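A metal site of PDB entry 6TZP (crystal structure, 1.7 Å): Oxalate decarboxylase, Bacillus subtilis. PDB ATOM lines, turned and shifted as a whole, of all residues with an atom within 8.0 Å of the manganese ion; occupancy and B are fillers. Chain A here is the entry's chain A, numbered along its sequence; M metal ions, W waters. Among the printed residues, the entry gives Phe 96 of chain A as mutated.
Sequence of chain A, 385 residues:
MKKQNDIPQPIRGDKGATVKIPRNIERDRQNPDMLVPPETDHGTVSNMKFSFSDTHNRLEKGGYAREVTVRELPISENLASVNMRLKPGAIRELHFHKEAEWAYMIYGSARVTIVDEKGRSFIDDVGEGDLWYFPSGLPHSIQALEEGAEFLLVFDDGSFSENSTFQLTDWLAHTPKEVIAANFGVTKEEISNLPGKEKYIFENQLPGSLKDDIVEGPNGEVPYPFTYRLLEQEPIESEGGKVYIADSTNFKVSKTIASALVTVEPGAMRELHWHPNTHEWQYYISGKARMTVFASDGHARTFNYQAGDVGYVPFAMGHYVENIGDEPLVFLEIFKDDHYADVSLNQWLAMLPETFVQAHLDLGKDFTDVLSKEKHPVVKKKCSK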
ATOM      1  N   MET A  84      19.633 -10.072   8.264  1.00  0.00           N
ATOM      2  CA  MET A  84      20.452 -10.336   9.444  1.00  0.00           C
ATOM      3  C   MET A  84      20.323  -9.199  10.449  1.00  0.00           C
ATOM      4  O   MET A  84      20.262  -8.016  10.077  1.00  0.00           O
ATOM      5  CB  MET A  84      21.929 -10.532   9.063  1.00  0.00           C
ATOM      6  CG  MET A  84      22.847 -10.812  10.251  1.00  0.00           C
ATOM      7  SD  MET A  84      24.472 -11.408   9.755  1.00  0.00           S
ATOM      8  CE  MET A  84      24.046 -13.082   9.259  1.00  0.00           C
ATOM      9  N   ARG A  92      29.246 -10.787  13.663  1.00  0.00           N
ATOM     10  CA  ARG A  92      29.119 -11.858  12.672  1.00  0.00           C
ATOM     11  C   ARG A  92      30.536 -12.320  12.350  1.00  0.00           C
ATOM     12  O   ARG A  92      31.338 -11.564  11.815  1.00  0.00           O
ATOM     13  CB  ARG A  92      28.375 -11.377  11.420  1.00  0.00           C
ATOM     14  CG  ARG A  92      28.376 -12.381  10.259  1.00  0.00           C
ATOM     15  CD  ARG A  92      27.513 -13.615  10.536  1.00  0.00           C
ATOM     16  NE  ARG A  92      27.530 -14.542   9.390  1.00  0.00           N
ATOM     17  CZ  ARG A  92      28.353 -15.579   9.277  1.00  0.00           C
ATOM     18  NH1 ARG A  92      29.221 -15.862  10.251  1.00  0.00           N
ATOM     19  NH2 ARG A  92      28.309 -16.357   8.193  1.00  0.00           N
ATOM     20  N   GLU A  93      30.824 -13.572  12.715  1.00  0.00           N
ATOM     21  CA  GLU A  93      32.174 -14.123  12.745  1.00  0.00           C
ATOM     22  C   GLU A  93      32.887 -13.980  11.409  1.00  0.00           C
ATOM     23  O   GLU A  93      32.315 -14.240  10.348  1.00  0.00           O
ATOM     24  CB  GLU A  93      32.098 -15.604  13.117  1.00  0.00           C
ATOM     25  CG  GLU A  93      33.451 -16.287  13.097  1.00  0.00           C
ATOM     26  CD  GLU A  93      33.415 -17.764  13.439  1.00  0.00           C
ATOM     27  OE1 GLU A  93      32.356 -18.315  13.801  1.00  0.00           O
ATOM     28  OE2 GLU A  93      34.487 -18.382  13.334  1.00  0.00           O
ATOM     29  N   LEU A  94      34.171 -13.606  11.468  1.00  0.00           N
ATOM     30  CA  LEU A  94      35.089 -13.627  10.335  1.00  0.00           C
ATOM     31  C   LEU A  94      34.875 -14.853   9.449  1.00  0.00           C
ATOM     32  O   LEU A  94      34.949 -15.991   9.920  1.00  0.00           O
ATOM     33  CB  LEU A  94      36.524 -13.601  10.865  1.00  0.00           C
ATOM     34  CG  LEU A  94      36.993 -12.243  11.396  1.00  0.00           C
ATOM     35  CD1 LEU A  94      38.186 -12.394  12.359  1.00  0.00           C
ATOM     36  CD2 LEU A  94      37.371 -11.360  10.223  1.00  0.00           C
ATOM     37  N   HIS A  95      34.622 -14.625   8.154  1.00  0.00           N
ATOM     38  CA  HIS A  95      34.214 -15.710   7.261  1.00  0.00           C
ATOM     39  C   HIS A  95      34.415 -15.291   5.807  1.00  0.00           C
ATOM     40  O   HIS A  95      34.714 -14.130   5.514  1.00  0.00           O
ATOM     41  CB  HIS A  95      32.739 -16.109   7.517  1.00  0.00           C
ATOM     42  CG  HIS A  95      31.739 -15.092   7.034  1.00  0.00           C
ATOM     43  ND1 HIS A  95      31.291 -14.045   7.821  1.00  0.00           N
ATOM     44  CD2 HIS A  95      31.103 -14.965   5.846  1.00  0.00           C
ATOM     45  CE1 HIS A  95      30.439 -13.310   7.131  1.00  0.00           C
ATOM     46  NE2 HIS A  95      30.306 -13.854   5.925  1.00  0.00           N
ATOM     47  N   PHE A  96      34.229 -16.246   4.905  1.00  0.00           N
ATOM     48  CA  PHE A  96      34.243 -15.954   3.474  1.00  0.00           C
ATOM     49  C   PHE A  96      33.346 -16.970   2.756  1.00  0.00           C
ATOM     50  O   PHE A  96      32.839 -17.911   3.375  1.00  0.00           O
ATOM     51  CB  PHE A  96      35.684 -15.974   2.908  1.00  0.00           C
ATOM     52  CG  PHE A  96      36.469 -17.226   3.239  1.00  0.00           C
ATOM     53  CD1 PHE A  96      37.157 -17.346   4.454  1.00  0.00           C
ATOM     54  CD2 PHE A  96      36.556 -18.270   2.326  1.00  0.00           C
ATOM     55  CE1 PHE A  96      37.892 -18.496   4.754  1.00  0.00           C
ATOM     56  CE2 PHE A  96      37.291 -19.420   2.627  1.00  0.00           C
ATOM     57  CZ  PHE A  96      37.950 -19.533   3.841  1.00  0.00           C
ATOM     58  N   HIS A  97      33.127 -16.741   1.460  1.00  0.00           N
ATOM     59  CA  HIS A  97      32.289 -17.639   0.672  1.00  0.00           C
ATOM     60  C   HIS A  97      32.570 -17.413  -0.809  1.00  0.00           C
ATOM     61  O   HIS A  97      33.166 -16.407  -1.196  1.00  0.00           O
ATOM     62  CB  HIS A  97      30.786 -17.444   0.952  1.00  0.00           C
ATOM     63  CG  HIS A  97      30.427 -16.058   1.368  1.00  0.00           C
ATOM     64  ND1 HIS A  97      30.470 -14.981   0.504  1.00  0.00           N
ATOM     65  CD2 HIS A  97      30.018 -15.565   2.561  1.00  0.00           C
ATOM     66  CE1 HIS A  97      30.111 -13.883   1.160  1.00  0.00           C
ATOM     67  NE2 HIS A  97      29.846 -14.209   2.406  1.00  0.00           N
ATOM     68  N   GLU A  99      30.426 -16.699  -3.149  1.00  0.00           N
ATOM     69  CA  GLU A  99      29.574 -15.676  -3.721  1.00  0.00           C
ATOM     70  C   GLU A  99      30.074 -14.282  -3.360  1.00  0.00           C
ATOM     71  O   GLU A  99      30.641 -14.076  -2.276  1.00  0.00           O
ATOM     72  CB  GLU A  99      28.143 -15.845  -3.231  1.00  0.00           C
ATOM     73  CG  GLU A  99      27.464 -17.125  -3.701  1.00  0.00           C
ATOM     74  CD  GLU A  99      27.841 -18.356  -2.867  1.00  0.00           C
ATOM     75  OE1 GLU A  99      28.571 -18.250  -1.869  1.00  0.00           O
ATOM     76  OE2 GLU A  99      27.373 -19.455  -3.226  1.00  0.00           O
ATOM     77  N   ALA A 100      29.860 -13.331  -4.265  1.00  0.00           N
ATOM     78  CA  ALA A 100      29.979 -11.934  -3.893  1.00  0.00           C
ATOM     79  C   ALA A 100      28.781 -11.541  -3.039  1.00  0.00           C
ATOM     80  O   ALA A 100      27.685 -12.117  -3.175  1.00  0.00           O
ATOM     81  CB  ALA A 100      30.055 -11.028  -5.124  1.00  0.00           C
ATOM     82  N   GLU A 101      28.989 -10.546  -2.180  1.00  0.00           N
ATOM     83  CA  GLU A 101      27.995 -10.124  -1.212  1.00  0.00           C
ATOM     84  C   GLU A 101      27.756  -8.621  -1.340  1.00  0.00           C
ATOM     85  O   GLU A 101      28.717  -7.842  -1.328  1.00  0.00           O
ATOM     86  CB  GLU A 101      28.438 -10.471   0.208  1.00  0.00           C
ATOM     87  CG  GLU A 101      27.630  -9.797   1.319  1.00  0.00           C
ATOM     88  CD  GLU A 101      28.088 -10.273   2.681  1.00  0.00           C
ATOM     89  OE1 GLU A 101      28.536 -11.440   2.751  1.00  0.00           O
ATOM     90  OE2 GLU A 101      28.031  -9.495   3.658  1.00  0.00           O
ATOM     91  N   TRP A 102      26.496  -8.228  -1.445  1.00  0.00           N
ATOM     92  CA  TRP A 102      26.077  -6.840  -1.459  1.00  0.00           C
ATOM     93  C   TRP A 102      25.155  -6.599  -0.269  1.00  0.00           C
ATOM     94  O   TRP A 102      24.400  -7.497   0.124  1.00  0.00           O
ATOM     95  CB  TRP A 102      25.342  -6.533  -2.768  1.00  0.00           C
ATOM     96  CG  TRP A 102      24.867  -5.115  -2.965  1.00  0.00           C
ATOM     97  CD1 TRP A 102      25.481  -4.128  -3.679  1.00  0.00           C
ATOM     98  CD2 TRP A 102      23.618  -4.561  -2.517  1.00  0.00           C
ATOM     99  NE1 TRP A 102      24.717  -2.993  -3.683  1.00  0.00           N
ATOM    100  CE2 TRP A 102      23.569  -3.228  -2.963  1.00  0.00           C
ATOM    101  CE3 TRP A 102      22.559  -5.068  -1.754  1.00  0.00           C
ATOM    102  CZ2 TRP A 102      22.506  -2.390  -2.679  1.00  0.00           C
ATOM    103  CZ3 TRP A 102      21.489  -4.227  -1.477  1.00  0.00           C
ATOM    104  CH2 TRP A 102      21.469  -2.904  -1.937  1.00  0.00           C
ATOM    105  N   TRP A 132      27.613  -2.000   1.400  1.00  0.00           N
ATOM    106  CA  TRP A 132      28.924  -2.582   1.170  1.00  0.00           C
ATOM    107  C   TRP A 132      28.829  -3.612   0.050  1.00  0.00           C
ATOM    108  O   TRP A 132      27.743  -4.053  -0.323  1.00  0.00           O
ATOM    109  CB  TRP A 132      29.546  -3.199   2.431  1.00  0.00           C
ATOM    110  CG  TRP A 132      28.919  -4.436   3.050  1.00  0.00           C
ATOM    111  CD1 TRP A 132      28.951  -5.722   2.571  1.00  0.00           C
ATOM    112  CD2 TRP A 132      28.255  -4.490   4.313  1.00  0.00           C
ATOM    113  NE1 TRP A 132      28.313  -6.564   3.462  1.00  0.00           N
ATOM    114  CE2 TRP A 132      27.890  -5.838   4.538  1.00  0.00           C
ATOM    115  CE3 TRP A 132      27.934  -3.534   5.286  1.00  0.00           C
ATOM    116  CZ2 TRP A 132      27.187  -6.240   5.680  1.00  0.00           C
ATOM    117  CZ3 TRP A 132      27.253  -3.940   6.422  1.00  0.00           C
ATOM    118  CH2 TRP A 132      26.888  -5.282   6.610  1.00  0.00           C
ATOM    119  N   PHE A 134      31.346  -7.056  -1.046  1.00  0.00           N
ATOM    120  CA  PHE A 134      32.533  -7.878  -0.826  1.00  0.00           C
ATOM    121  C   PHE A 134      32.705  -8.797  -2.025  1.00  0.00           C
ATOM    122  O   PHE A 134      31.846  -9.658  -2.253  1.00  0.00           O
ATOM    123  CB  PHE A 134      32.397  -8.686   0.462  1.00  0.00           C
ATOM    124  CG  PHE A 134      32.200  -7.853   1.704  1.00  0.00           C
ATOM    125  CD1 PHE A 134      32.762  -6.583   1.797  1.00  0.00           C
ATOM    126  CD2 PHE A 134      31.451  -8.347   2.768  1.00  0.00           C
ATOM    127  CE1 PHE A 134      32.576  -5.811   2.942  1.00  0.00           C
ATOM    128  CE2 PHE A 134      31.265  -7.572   3.926  1.00  0.00           C
ATOM    129  CZ  PHE A 134      31.828  -6.305   4.006  1.00  0.00           C
ATOM    130  N   LEU A 138      36.645 -12.930  -0.704  1.00  0.00           N
ATOM    131  CA  LEU A 138      37.482 -12.145   0.203  1.00  0.00           C
ATOM    132  C   LEU A 138      36.883 -12.156   1.617  1.00  0.00           C
ATOM    133  O   LEU A 138      35.664 -12.051   1.773  1.00  0.00           O
ATOM    134  CB  LEU A 138      37.609 -10.705  -0.277  1.00  0.00           C
ATOM    135  CG  LEU A 138      38.287 -10.557  -1.650  1.00  0.00           C
ATOM    136  CD1 LEU A 138      38.443  -9.080  -2.008  1.00  0.00           C
ATOM    137  CD2 LEU A 138      39.634 -11.280  -1.706  1.00  0.00           C
ATOM    138  N   PRO A 139      37.719 -12.326   2.630  1.00  0.00           N
ATOM    139  CA  PRO A 139      37.212 -12.579   3.989  1.00  0.00           C
ATOM    140  C   PRO A 139      36.808 -11.296   4.695  1.00  0.00           C
ATOM    141  O   PRO A 139      37.436 -10.248   4.537  1.00  0.00           O
ATOM    142  CB  PRO A 139      38.402 -13.239   4.677  1.00  0.00           C
ATOM    143  CG  PRO A 139      39.603 -12.565   4.021  1.00  0.00           C
ATOM    144  CD  PRO A 139      39.193 -12.392   2.565  1.00  0.00           C
ATOM    145  N   HIS A 140      35.762 -11.401   5.513  1.00  0.00           N
ATOM    146  CA  HIS A 140      35.144 -10.206   6.078  1.00  0.00           C
ATOM    147  C   HIS A 140      34.447 -10.534   7.387  1.00  0.00           C
ATOM    148  O   HIS A 140      34.289 -11.700   7.780  1.00  0.00           O
ATOM    149  CB  HIS A 140      34.163  -9.569   5.083  1.00  0.00           C
ATOM    150  CG  HIS A 140      33.157 -10.524   4.514  1.00  0.00           C
ATOM    151  ND1 HIS A 140      33.407 -11.298   3.398  1.00  0.00           N
ATOM    152  CD2 HIS A 140      31.901 -10.827   4.909  1.00  0.00           C
ATOM    153  CE1 HIS A 140      32.336 -12.025   3.121  1.00  0.00           C
ATOM    154  NE2 HIS A 140      31.408 -11.767   4.030  1.00  0.00           N
ATOM    155  N   SER A 141      34.026  -9.474   8.079  1.00  0.00           N
ATOM    156  CA  SER A 141      33.311  -9.566   9.343  1.00  0.00           C
ATOM    157  C   SER A 141      32.397  -8.356   9.472  1.00  0.00           C
ATOM    158  O   SER A 141      32.554  -7.368   8.749  1.00  0.00           O
ATOM    159  CB  SER A 141      34.297  -9.641  10.510  1.00  0.00           C
ATOM    160  OG  SER A 141      34.959  -8.379  10.669  1.00  0.00           O
ATOM    161  N   ILE A 142      31.404  -8.458  10.368  1.00  0.00           N
ATOM    162  CA  ILE A 142      30.485  -7.371  10.682  1.00  0.00           C
ATOM    163  C   ILE A 142      30.364  -7.297  12.198  1.00  0.00           C
ATOM    164  O   ILE A 142      30.241  -8.333  12.848  1.00  0.00           O
ATOM    165  CB  ILE A 142      29.065  -7.602  10.078  1.00  0.00           C
ATOM    166  CG1 ILE A 142      29.111  -8.065   8.627  1.00  0.00           C
ATOM    167  CG2 ILE A 142      28.191  -6.343  10.220  1.00  0.00           C
ATOM    168  CD1 ILE A 142      27.855  -8.853   8.263  1.00  0.00           C
ATOM    169  N   LEU A 153      21.319  -8.582   3.063  1.00  0.00           N
ATOM    170  CA  LEU A 153      22.440  -9.083   2.271  1.00  0.00           C
ATOM    171  C   LEU A 153      21.909  -9.713   0.990  1.00  0.00           C
ATOM    172  O   LEU A 153      20.877 -10.391   1.006  1.00  0.00           O
ATOM    173  CB  LEU A 153      23.243 -10.109   3.066  1.00  0.00           C
ATOM    174  CG  LEU A 153      23.706  -9.693   4.468  1.00  0.00           C
ATOM    175  CD1 LEU A 153      24.374 -10.888   5.164  1.00  0.00           C
ATOM    176  CD2 LEU A 153      24.650  -8.514   4.400  1.00  0.00           C
ATOM    177  N   PHE A 155      23.367 -12.094  -2.329  1.00  0.00           N
ATOM    178  CA  PHE A 155      24.478 -12.913  -2.804  1.00  0.00           C
ATOM    179  C   PHE A 155      24.245 -13.297  -4.258  1.00  0.00           C
ATOM    180  O   PHE A 155      23.102 -13.592  -4.639  1.00  0.00           O
ATOM    181  CB  PHE A 155      24.631 -14.182  -1.939  1.00  0.00           C
ATOM    182  CG  PHE A 155      24.809 -13.871  -0.495  1.00  0.00           C
ATOM    183  CD1 PHE A 155      26.071 -13.658   0.028  1.00  0.00           C
ATOM    184  CD2 PHE A 155      23.705 -13.750   0.345  1.00  0.00           C
ATOM    185  CE1 PHE A 155      26.247 -13.338   1.370  1.00  0.00           C
ATOM    186  CE2 PHE A 155      23.863 -13.418   1.693  1.00  0.00           C
ATOM    187  CZ  PHE A 155      25.143 -13.218   2.210  1.00  0.00           C
ATOM    188  N   PHE A 160      22.808 -20.061  -2.611  1.00  0.00           N
ATOM    189  CA  PHE A 160      23.536 -19.731  -1.385  1.00  0.00           C
ATOM    190  C   PHE A 160      22.748 -20.157  -0.144  1.00  0.00           C
ATOM    191  O   PHE A 160      21.519 -20.221  -0.162  1.00  0.00           O
ATOM    192  CB  PHE A 160      23.796 -18.220  -1.348  1.00  0.00           C
ATOM    193  CG  PHE A 160      24.532 -17.736  -0.111  1.00  0.00           C
ATOM    194  CD1 PHE A 160      25.916 -17.816  -0.043  1.00  0.00           C
ATOM    195  CD2 PHE A 160      23.836 -17.182   0.947  1.00  0.00           C
ATOM    196  CE1 PHE A 160      26.605 -17.368   1.086  1.00  0.00           C
ATOM    197  CE2 PHE A 160      24.519 -16.742   2.077  1.00  0.00           C
ATOM    198  CZ  PHE A 160      25.897 -16.820   2.137  1.00  0.00           C
ATOM    199  N   GLU A 162      23.329 -19.062   4.184  1.00  0.00           N
ATOM    200  CA  GLU A 162      24.185 -18.453   5.198  1.00  0.00           C
ATOM    201  C   GLU A 162      24.697 -19.479   6.198  1.00  0.00           C
ATOM    202  O   GLU A 162      25.684 -19.208   6.894  1.00  0.00           O
ATOM    203  CB  GLU A 162      23.445 -17.328   5.941  1.00  0.00           C
ATOM    204  CG  GLU A 162      24.304 -16.465   6.886  1.00  0.00           C
ATOM    205  CD  GLU A 162      25.171 -15.432   6.161  1.00  0.00           C
ATOM    206  OE1 GLU A 162      24.872 -15.126   4.997  1.00  0.00           O
ATOM    207  OE2 GLU A 162      26.138 -14.921   6.761  1.00  0.00           O
ATOM    208  N   THR A 165      28.786 -20.808   5.074  1.00  0.00           N
ATOM    209  CA  THR A 165      29.962 -19.981   4.852  1.00  0.00           C
ATOM    210  C   THR A 165      31.197 -20.679   5.424  1.00  0.00           C
ATOM    211  O   THR A 165      31.086 -21.625   6.218  1.00  0.00           O
ATOM    212  CB  THR A 165      29.774 -18.613   5.484  1.00  0.00           C
ATOM    213  OG1 THR A 165      29.853 -18.727   6.906  1.00  0.00           O
ATOM    214  CG2 THR A 165      28.412 -18.042   5.100  1.00  0.00           C
HETATM  215 MN    MN M   1      29.404 -12.748   4.215  1.00  0.00          MN
HETATM  216  O   HOH W   1      27.486 -14.046   4.523  1.00  0.00           O
HETATM  217  O   HOH W   2      28.671 -11.157   5.706  1.00  0.00           O
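N of Phe 134 is in hydrogen-bond range of O of Glu 101 (2.8 Å).
The side-chain carboxylate of Glu 101 lies within hydrogen-bond range of the indole nitrogen of Trp 132.
ND1 of His 95 is in hydrogen-bond range of O of Glu 93, 2.7 Å away.
The backbone carbonyl oxygen of Leu 138 is in hydrogen-bond range of a ring nitrogen (ND1) of His 140 (2.9 Å).
The backbone carbonyl oxygen (O) of Glu 99 lies within hydrogen-bond range of a ring nitrogen (ND1) of His 97 (2.9 Å).
Of the 23 residues printed, 4 come within 4 Å of the manganese ion.
Along chain A the residues within 4 Å of the manganese ion span positions 95 to 140.
The manganese ion is bound by OE1 of Glu 101, 2.1 Å away.
The manganese ion is bound by NE2 of His 95, at 2.2 Å.
NE2 of His 140 binds the manganese ion, 2.2 Å away.
Water W2 is bound to the manganese ion (2.3 Å).
Water W1 binds the manganese ion (2.3 Å).
The manganese ion is bound by a ring nitrogen (NE2) of His 97 (2.4 Å).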
